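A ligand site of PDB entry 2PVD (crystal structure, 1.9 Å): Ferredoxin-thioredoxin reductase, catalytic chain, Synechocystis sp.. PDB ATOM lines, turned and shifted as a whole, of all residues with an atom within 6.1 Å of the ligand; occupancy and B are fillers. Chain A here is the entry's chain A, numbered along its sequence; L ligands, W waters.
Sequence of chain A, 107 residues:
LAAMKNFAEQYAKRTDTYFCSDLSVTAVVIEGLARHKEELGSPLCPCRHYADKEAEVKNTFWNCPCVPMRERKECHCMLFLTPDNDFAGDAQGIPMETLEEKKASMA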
ATOM      1  N   PHE A   7     -23.802 -10.533  -7.273  1.00  0.00           N
ATOM      2  CA  PHE A   7     -23.629 -11.961  -7.087  1.00  0.00           C
ATOM      3  C   PHE A   7     -24.910 -12.644  -6.607  1.00  0.00           C
ATOM      4  O   PHE A   7     -25.342 -13.652  -7.170  1.00  0.00           O
ATOM      5  CB  PHE A   7     -22.511 -12.254  -6.079  1.00  0.00           C
ATOM      6  CG  PHE A   7     -22.671 -13.587  -5.392  1.00  0.00           C
ATOM      7  CD1 PHE A   7     -22.608 -14.775  -6.119  1.00  0.00           C
ATOM      8  CD2 PHE A   7     -22.987 -13.644  -4.035  1.00  0.00           C
ATOM      9  CE1 PHE A   7     -22.852 -16.001  -5.511  1.00  0.00           C
ATOM     10  CE2 PHE A   7     -23.240 -14.861  -3.419  1.00  0.00           C
ATOM     11  CZ  PHE A   7     -23.175 -16.046  -4.159  1.00  0.00           C
ATOM     12  N   TYR A  11     -27.050 -15.404  -8.732  1.00  0.00           N
ATOM     13  CA  TYR A  11     -27.109 -16.763  -8.204  1.00  0.00           C
ATOM     14  C   TYR A  11     -28.551 -17.163  -7.944  1.00  0.00           C
ATOM     15  O   TYR A  11     -28.951 -18.304  -8.187  1.00  0.00           O
ATOM     16  CB  TYR A  11     -26.305 -16.870  -6.913  1.00  0.00           C
ATOM     17  CG  TYR A  11     -26.072 -18.311  -6.515  1.00  0.00           C
ATOM     18  CD1 TYR A  11     -25.240 -19.130  -7.290  1.00  0.00           C
ATOM     19  CD2 TYR A  11     -26.705 -18.862  -5.406  1.00  0.00           C
ATOM     20  CE1 TYR A  11     -25.054 -20.476  -6.967  1.00  0.00           C
ATOM     21  CE2 TYR A  11     -26.520 -20.212  -5.070  1.00  0.00           C
ATOM     22  CZ  TYR A  11     -25.701 -21.008  -5.856  1.00  0.00           C
ATOM     23  OH  TYR A  11     -25.529 -22.342  -5.563  1.00  0.00           O
ATOM     24  N   VAL A  29     -27.604  -9.724   5.180  1.00  0.00           N
ATOM     25  CA  VAL A  29     -26.714 -10.829   4.814  1.00  0.00           C
ATOM     26  C   VAL A  29     -25.731 -10.426   3.724  1.00  0.00           C
ATOM     27  O   VAL A  29     -24.557 -10.758   3.794  1.00  0.00           O
ATOM     28  CB  VAL A  29     -27.526 -12.068   4.342  1.00  0.00           C
ATOM     29  CG1 VAL A  29     -26.566 -13.229   4.049  1.00  0.00           C
ATOM     30  CG2 VAL A  29     -28.529 -12.469   5.422  1.00  0.00           C
ATOM     31  N   LEU A  33     -21.781 -10.455   3.941  1.00  0.00           N
ATOM     32  CA  LEU A  33     -20.948 -11.218   3.017  1.00  0.00           C
ATOM     33  C   LEU A  33     -19.874 -10.276   2.485  1.00  0.00           C
ATOM     34  O   LEU A  33     -18.698 -10.597   2.456  1.00  0.00           O
ATOM     35  CB  LEU A  33     -21.785 -11.761   1.857  1.00  0.00           C
ATOM     36  CG  LEU A  33     -22.707 -12.968   2.100  1.00  0.00           C
ATOM     37  CD1 LEU A  33     -23.610 -13.175   0.900  1.00  0.00           C
ATOM     38  CD2 LEU A  33     -21.869 -14.208   2.378  1.00  0.00           C
ATOM     39  N   PRO A  43     -16.180 -14.683   0.652  1.00  0.00           N
ATOM     40  CA  PRO A  43     -17.547 -14.432   1.125  1.00  0.00           C
ATOM     41  C   PRO A  43     -18.004 -15.420   2.219  1.00  0.00           C
ATOM     42  O   PRO A  43     -19.044 -16.063   2.082  1.00  0.00           O
ATOM     43  CB  PRO A  43     -18.402 -14.575  -0.141  1.00  0.00           C
ATOM     44  CG  PRO A  43     -17.416 -14.503  -1.281  1.00  0.00           C
ATOM     45  CD  PRO A  43     -16.204 -15.196  -0.733  1.00  0.00           C
ATOM     46  N   LEU A  44     -17.232 -15.522   3.300  1.00  0.00           N
ATOM     47  CA  LEU A  44     -17.605 -16.420   4.391  1.00  0.00           C
ATOM     48  C   LEU A  44     -18.996 -16.062   4.920  1.00  0.00           C
ATOM     49  O   LEU A  44     -19.298 -14.879   5.137  1.00  0.00           O
ATOM     50  CB  LEU A  44     -16.571 -16.317   5.524  1.00  0.00           C
ATOM     51  CG  LEU A  44     -16.722 -17.243   6.726  1.00  0.00           C
ATOM     52  CD1 LEU A  44     -16.699 -18.700   6.279  1.00  0.00           C
ATOM     53  CD2 LEU A  44     -15.591 -16.980   7.720  1.00  0.00           C
ATOM     54  N   CYS A  45     -19.838 -17.068   5.118  1.00  0.00           N
ATOM     55  CA  CYS A  45     -21.188 -16.821   5.615  1.00  0.00           C
ATOM     56  C   CYS A  45     -21.103 -15.964   6.873  1.00  0.00           C
ATOM     57  O   CYS A  45     -20.395 -16.306   7.810  1.00  0.00           O
ATOM     58  CB  CYS A  45     -21.926 -18.125   5.933  1.00  0.00           C
ATOM     59  SG  CYS A  45     -23.672 -17.852   6.348  1.00  0.00           S
ATOM     60  N   PRO A  46     -21.831 -14.848   6.901  1.00  0.00           N
ATOM     61  CA  PRO A  46     -21.816 -13.948   8.046  1.00  0.00           C
ATOM     62  C   PRO A  46     -22.840 -14.287   9.115  1.00  0.00           C
ATOM     63  O   PRO A  46     -22.817 -13.701  10.200  1.00  0.00           O
ATOM     64  CB  PRO A  46     -22.090 -12.604   7.408  1.00  0.00           C
ATOM     65  CG  PRO A  46     -23.158 -12.964   6.418  1.00  0.00           C
ATOM     66  CD  PRO A  46     -22.649 -14.272   5.813  1.00  0.00           C
ATOM     67  N   CYS A  47     -23.732 -15.230   8.826  1.00  0.00           N
ATOM     68  CA  CYS A  47     -24.761 -15.580   9.796  1.00  0.00           C
ATOM     69  C   CYS A  47     -24.419 -16.777  10.668  1.00  0.00           C
ATOM     70  O   CYS A  47     -25.297 -17.544  11.066  1.00  0.00           O
ATOM     71  CB  CYS A  47     -26.086 -15.811   9.070  1.00  0.00           C
ATOM     72  SG  CYS A  47     -26.667 -14.347   8.180  1.00  0.00           S
ATOM     73  N   TRP A  62     -17.977 -23.054   4.079  1.00  0.00           N
ATOM     74  CA  TRP A  62     -18.899 -21.957   4.313  1.00  0.00           C
ATOM     75  C   TRP A  62     -18.728 -20.700   3.473  1.00  0.00           C
ATOM     76  O   TRP A  62     -19.331 -19.671   3.774  1.00  0.00           O
ATOM     77  CB  TRP A  62     -18.908 -21.582   5.794  1.00  0.00           C
ATOM     78  CG  TRP A  62     -19.610 -22.581   6.661  1.00  0.00           C
ATOM     79  CD1 TRP A  62     -19.079 -23.316   7.674  1.00  0.00           C
ATOM     80  CD2 TRP A  62     -21.004 -22.926   6.604  1.00  0.00           C
ATOM     81  NE1 TRP A  62     -20.042 -24.093   8.261  1.00  0.00           N
ATOM     82  CE2 TRP A  62     -21.239 -23.869   7.627  1.00  0.00           C
ATOM     83  CE3 TRP A  62     -22.072 -22.517   5.790  1.00  0.00           C
ATOM     84  CZ2 TRP A  62     -22.508 -24.423   7.867  1.00  0.00           C
ATOM     85  CZ3 TRP A  62     -23.341 -23.071   6.030  1.00  0.00           C
ATOM     86  CH2 TRP A  62     -23.543 -24.011   7.059  1.00  0.00           C
ATOM     87  N   ASN A  63     -17.888 -20.756   2.434  1.00  0.00           N
ATOM     88  CA  ASN A  63     -17.753 -19.583   1.577  1.00  0.00           C
ATOM     89  C   ASN A  63     -18.993 -19.594   0.701  1.00  0.00           C
ATOM     90  O   ASN A  63     -19.290 -20.599   0.065  1.00  0.00           O
ATOM     91  CB  ASN A  63     -16.484 -19.664   0.721  1.00  0.00           C
ATOM     92  CG  ASN A  63     -15.216 -19.486   1.542  1.00  0.00           C
ATOM     93  OD1 ASN A  63     -15.240 -18.831   2.591  1.00  0.00           O
ATOM     94  ND2 ASN A  63     -14.114 -20.037   1.062  1.00  0.00           N
ATOM     95  N   CYS A  64     -19.731 -18.491   0.680  1.00  0.00           N
ATOM     96  CA  CYS A  64     -20.974 -18.385  -0.089  1.00  0.00           C
ATOM     97  C   CYS A  64     -20.711 -18.373  -1.590  1.00  0.00           C
ATOM     98  O   CYS A  64     -19.816 -17.669  -2.058  1.00  0.00           O
ATOM     99  CB  CYS A  64     -21.730 -17.112   0.328  1.00  0.00           C
ATOM    100  SG  CYS A  64     -23.428 -16.909  -0.328  1.00  0.00           S
ATOM    101  N   PRO A  65     -21.463 -19.190  -2.364  1.00  0.00           N
ATOM    102  CA  PRO A  65     -22.514 -20.117  -1.913  1.00  0.00           C
ATOM    103  C   PRO A  65     -21.902 -21.359  -1.262  1.00  0.00           C
ATOM    104  O   PRO A  65     -21.084 -22.037  -1.861  1.00  0.00           O
ATOM    105  CB  PRO A  65     -23.278 -20.410  -3.204  1.00  0.00           C
ATOM    106  CG  PRO A  65     -22.206 -20.341  -4.257  1.00  0.00           C
ATOM    107  CD  PRO A  65     -21.430 -19.095  -3.833  1.00  0.00           C
ATOM    108  N   CYS A  66     -22.309 -21.631  -0.025  1.00  0.00           N
ATOM    109  CA  CYS A  66     -21.784 -22.745   0.757  1.00  0.00           C
ATOM    110  C   CYS A  66     -22.172 -24.127   0.236  1.00  0.00           C
ATOM    111  O   CYS A  66     -23.018 -24.260  -0.652  1.00  0.00           O
ATOM    112  CB  CYS A  66     -22.271 -22.621   2.199  1.00  0.00           C
ATOM    113  SG  CYS A  66     -24.071 -22.673   2.300  1.00  0.00           S
ATOM    114  N   VAL A  67     -21.537 -25.156   0.805  1.00  0.00           N
ATOM    115  CA  VAL A  67     -21.798 -26.534   0.409  1.00  0.00           C
ATOM    116  C   VAL A  67     -23.283 -26.912   0.520  1.00  0.00           C
ATOM    117  O   VAL A  67     -23.847 -27.491  -0.412  1.00  0.00           O
ATOM    118  CB  VAL A  67     -20.945 -27.531   1.242  1.00  0.00           C
ATOM    119  CG1 VAL A  67     -21.453 -28.958   1.050  1.00  0.00           C
ATOM    120  CG2 VAL A  67     -19.451 -27.448   0.804  1.00  0.00           C
ATOM    121  N   PRO A  68     -23.932 -26.596   1.654  1.00  0.00           N
ATOM    122  CA  PRO A  68     -25.346 -26.938   1.807  1.00  0.00           C
ATOM    123  C   PRO A  68     -26.223 -26.281   0.734  1.00  0.00           C
ATOM    124  O   PRO A  68     -27.202 -26.858   0.284  1.00  0.00           O
ATOM    125  CB  PRO A  68     -25.654 -26.437   3.207  1.00  0.00           C
ATOM    126  CG  PRO A  68     -24.355 -26.678   3.935  1.00  0.00           C
ATOM    127  CD  PRO A  68     -23.350 -26.153   2.933  1.00  0.00           C
ATOM    128  N   MET A  69     -25.854 -25.068   0.320  1.00  0.00           N
ATOM    129  CA  MET A  69     -26.643 -24.379  -0.686  1.00  0.00           C
ATOM    130  C   MET A  69     -26.352 -24.935  -2.087  1.00  0.00           C
ATOM    131  O   MET A  69     -27.276 -25.149  -2.874  1.00  0.00           O
ATOM    132  CB  MET A  69     -26.371 -22.879  -0.643  1.00  0.00           C
ATOM    133  CG  MET A  69     -27.148 -22.063  -1.679  1.00  0.00           C
ATOM    134  SD  MET A  69     -28.915 -22.209  -1.468  1.00  0.00           S
ATOM    135  CE  MET A  69     -29.519 -21.833  -3.159  1.00  0.00           C
ATOM    136  N   GLU A  74     -29.918 -25.413   0.369  1.00  0.00           N
ATOM    137  CA  GLU A  74     -30.236 -25.047   1.746  1.00  0.00           C
ATOM    138  C   GLU A  74     -29.424 -23.838   2.212  1.00  0.00           C
ATOM    139  O   GLU A  74     -28.197 -23.902   2.306  1.00  0.00           O
ATOM    140  CB  GLU A  74     -29.963 -26.241   2.681  1.00  0.00           C
ATOM    141  CG  GLU A  74     -31.094 -27.264   2.753  1.00  0.00           C
ATOM    142  CD  GLU A  74     -30.670 -28.561   3.419  1.00  0.00           C
ATOM    143  OE1 GLU A  74     -29.807 -28.498   4.325  1.00  0.00           O
ATOM    144  OE2 GLU A  74     -31.194 -29.632   3.054  1.00  0.00           O
ATOM    145  N   CYS A  75     -30.110 -22.744   2.506  1.00  0.00           N
ATOM    146  CA  CYS A  75     -29.474 -21.523   2.982  1.00  0.00           C
ATOM    147  C   CYS A  75     -30.112 -21.149   4.314  1.00  0.00           C
ATOM    148  O   CYS A  75     -31.172 -20.535   4.346  1.00  0.00           O
ATOM    149  CB  CYS A  75     -29.685 -20.388   1.971  1.00  0.00           C
ATOM    150  SG  CYS A  75     -28.972 -18.793   2.475  1.00  0.00           S
ATOM    151  N   HIS A  76     -29.459 -21.512   5.421  1.00  0.00           N
ATOM    152  CA  HIS A  76     -30.009 -21.224   6.749  1.00  0.00           C
ATOM    153  C   HIS A  76     -30.119 -19.722   7.038  1.00  0.00           C
ATOM    154  O   HIS A  76     -30.835 -19.319   7.953  1.00  0.00           O
ATOM    155  CB  HIS A  76     -29.167 -21.926   7.828  1.00  0.00           C
ATOM    156  CG  HIS A  76     -27.839 -21.271   8.082  1.00  0.00           C
ATOM    157  ND1 HIS A  76     -27.682 -20.260   8.997  1.00  0.00           N
ATOM    158  CD2 HIS A  76     -26.623 -21.465   7.508  1.00  0.00           C
ATOM    159  CE1 HIS A  76     -26.418 -19.849   8.982  1.00  0.00           C
ATOM    160  NE2 HIS A  76     -25.763 -20.566   8.083  1.00  0.00           N
ATOM    161  N   CYS A  77     -29.437 -18.896   6.240  1.00  0.00           N
ATOM    162  CA  CYS A  77     -29.436 -17.422   6.372  1.00  0.00           C
ATOM    163  C   CYS A  77     -30.721 -16.777   5.882  1.00  0.00           C
ATOM    164  O   CYS A  77     -31.029 -15.638   6.241  1.00  0.00           O
ATOM    165  CB  CYS A  77     -28.335 -16.780   5.537  1.00  0.00           C
ATOM    166  SG  CYS A  77     -26.706 -16.884   6.151  1.00  0.00           S
ATOM    167  N   MET A  78     -31.424 -17.475   5.011  1.00  0.00           N
ATOM    168  CA  MET A  78     -32.620 -16.943   4.415  1.00  0.00           C
ATOM    169  C   MET A  78     -32.239 -15.878   3.377  1.00  0.00           C
ATOM    170  O   MET A  78     -32.892 -14.835   3.255  1.00  0.00           O
ATOM    171  CB  MET A  78     -33.543 -16.352   5.484  1.00  0.00           C
ATOM    172  CG  MET A  78     -34.184 -17.417   6.362  1.00  0.00           C
ATOM    173  SD  MET A  78     -35.499 -16.773   7.414  1.00  0.00           S
ATOM    174  CE  MET A  78     -36.341 -15.658   6.301  1.00  0.00           C
ATOM    175  N   LEU A  79     -31.152 -16.154   2.654  1.00  0.00           N
ATOM    176  CA  LEU A  79     -30.726 -15.259   1.571  1.00  0.00           C
ATOM    177  C   LEU A  79     -31.338 -15.856   0.305  1.00  0.00           C
ATOM    178  O   LEU A  79     -32.050 -15.172  -0.426  1.00  0.00           O
ATOM    179  CB  LEU A  79     -29.198 -15.208   1.440  1.00  0.00           C
ATOM    180  CG  LEU A  79     -28.703 -14.353   0.258  1.00  0.00           C
ATOM    181  CD1 LEU A  79     -29.332 -12.947   0.351  1.00  0.00           C
ATOM    182  CD2 LEU A  79     -27.173 -14.255   0.262  1.00  0.00           C
ATOM    183  N   PHE A  80     -31.089 -17.140   0.072  1.00  0.00           N
ATOM    184  CA  PHE A  80     -31.633 -17.823  -1.092  1.00  0.00           C
ATOM    185  C   PHE A  80     -32.716 -18.809  -0.615  1.00  0.00           C
ATOM    186  O   PHE A  80     -32.410 -19.829   0.005  1.00  0.00           O
ATOM    187  CB  PHE A  80     -30.517 -18.568  -1.832  1.00  0.00           C
ATOM    188  CG  PHE A  80     -29.335 -17.702  -2.201  1.00  0.00           C
ATOM    189  CD1 PHE A  80     -28.084 -17.944  -1.643  1.00  0.00           C
ATOM    190  CD2 PHE A  80     -29.466 -16.648  -3.114  1.00  0.00           C
ATOM    191  CE1 PHE A  80     -26.974 -17.167  -2.000  1.00  0.00           C
ATOM    192  CE2 PHE A  80     -28.366 -15.872  -3.480  1.00  0.00           C
ATOM    193  CZ  PHE A  80     -27.119 -16.128  -2.926  1.00  0.00           C
HETATM  194 FE1  LIG L   1     -24.469 -18.016   1.406  1.00  0.00          FE
HETATM  195 FE2  LIG L   1     -24.778 -20.490   2.536  1.00  0.00          FE
HETATM  196 FE3  LIG L   1     -26.805 -18.792   2.556  1.00  0.00          FE
HETATM  197 FE4  LIG L   1     -24.677 -18.344   4.137  1.00  0.00          FE
HETATM  198  S1  LIG L   1     -26.163 -20.100   4.327  1.00  0.00           S
HETATM  199  S2  LIG L   1     -25.750 -16.760   2.839  1.00  0.00           S
HETATM  200  S3  LIG L   1     -22.969 -19.075   2.772  1.00  0.00           S
HETATM  201  S4  LIG L   1     -25.847 -19.709   0.674  1.00  0.00           S
HETATM  202  O   HOH W   1     -26.958 -23.314   4.833  1.00  0.00           O
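Residues that only touch the ligand: Met 69 (3.5 Å), Phe 80 (3.7 Å), Trp 62 (3.8 Å), Val 29 (3.8 Å) and Leu 79 (3.9 Å).
Hydrophobic or aromatic side chains that line the ligand: Val 29, Met 69, His 76, Leu 79 and Phe 80.
Of the 24 residues printed, 11 come within 4 Å of the ligand.
The backbone NH of Met 69 lies close to the side-chain sulfur of Cys 66 (3.6 Å).
The backbone carbonyl oxygen (O) of Pro 43 sits at hydrogen-bond distance from the backbone NH (N) of Cys 64 (2.9 Å).
The backbone NH (N) of Met 69 lies within hydrogen-bond range of the backbone carbonyl oxygen (O) of Glu 74.
N of Phe 80 sits close to SG of Cys 75.
SG of Cys 75 lies close to N of Leu 79, 3.4 Å away.
SG of Cys 45 lies close to N of Cys 47 (3.6 Å).
SG of Cys 47 sits close to SG of Cys 77.
SG of Cys 45 sits close to SG of Cys 77 (3.2 Å).
Water W1 lies within hydrogen-bond range of the backbone carbonyl oxygen of Glu 74 (2.9 Å), the backbone NH of His 76 (3.1 Å) and a sulfur (S1) of the ligand (3.3 Å).
FE3 of the ligand is bound by SG of Cys 75 (2.2 Å).
The backbone NH (N) of His 76 lies close to a sulfur (S1) of the ligand (3.7 Å).
The side-chain sulfur of Cys 45 binds an iron atom (FE4) of the ligand, at 2.5 Å.
SG of Cys 64 binds FE1 of the ligand (2.3 Å).
An iron atom (FE2) of the ligand is bound by the side-chain sulfur (SG) of Cys 66 (2.3 Å).
The side-chain sulfur (SG) of Cys 77 sits close to a sulfur (S2) of the ligand, 3.4 Å away.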
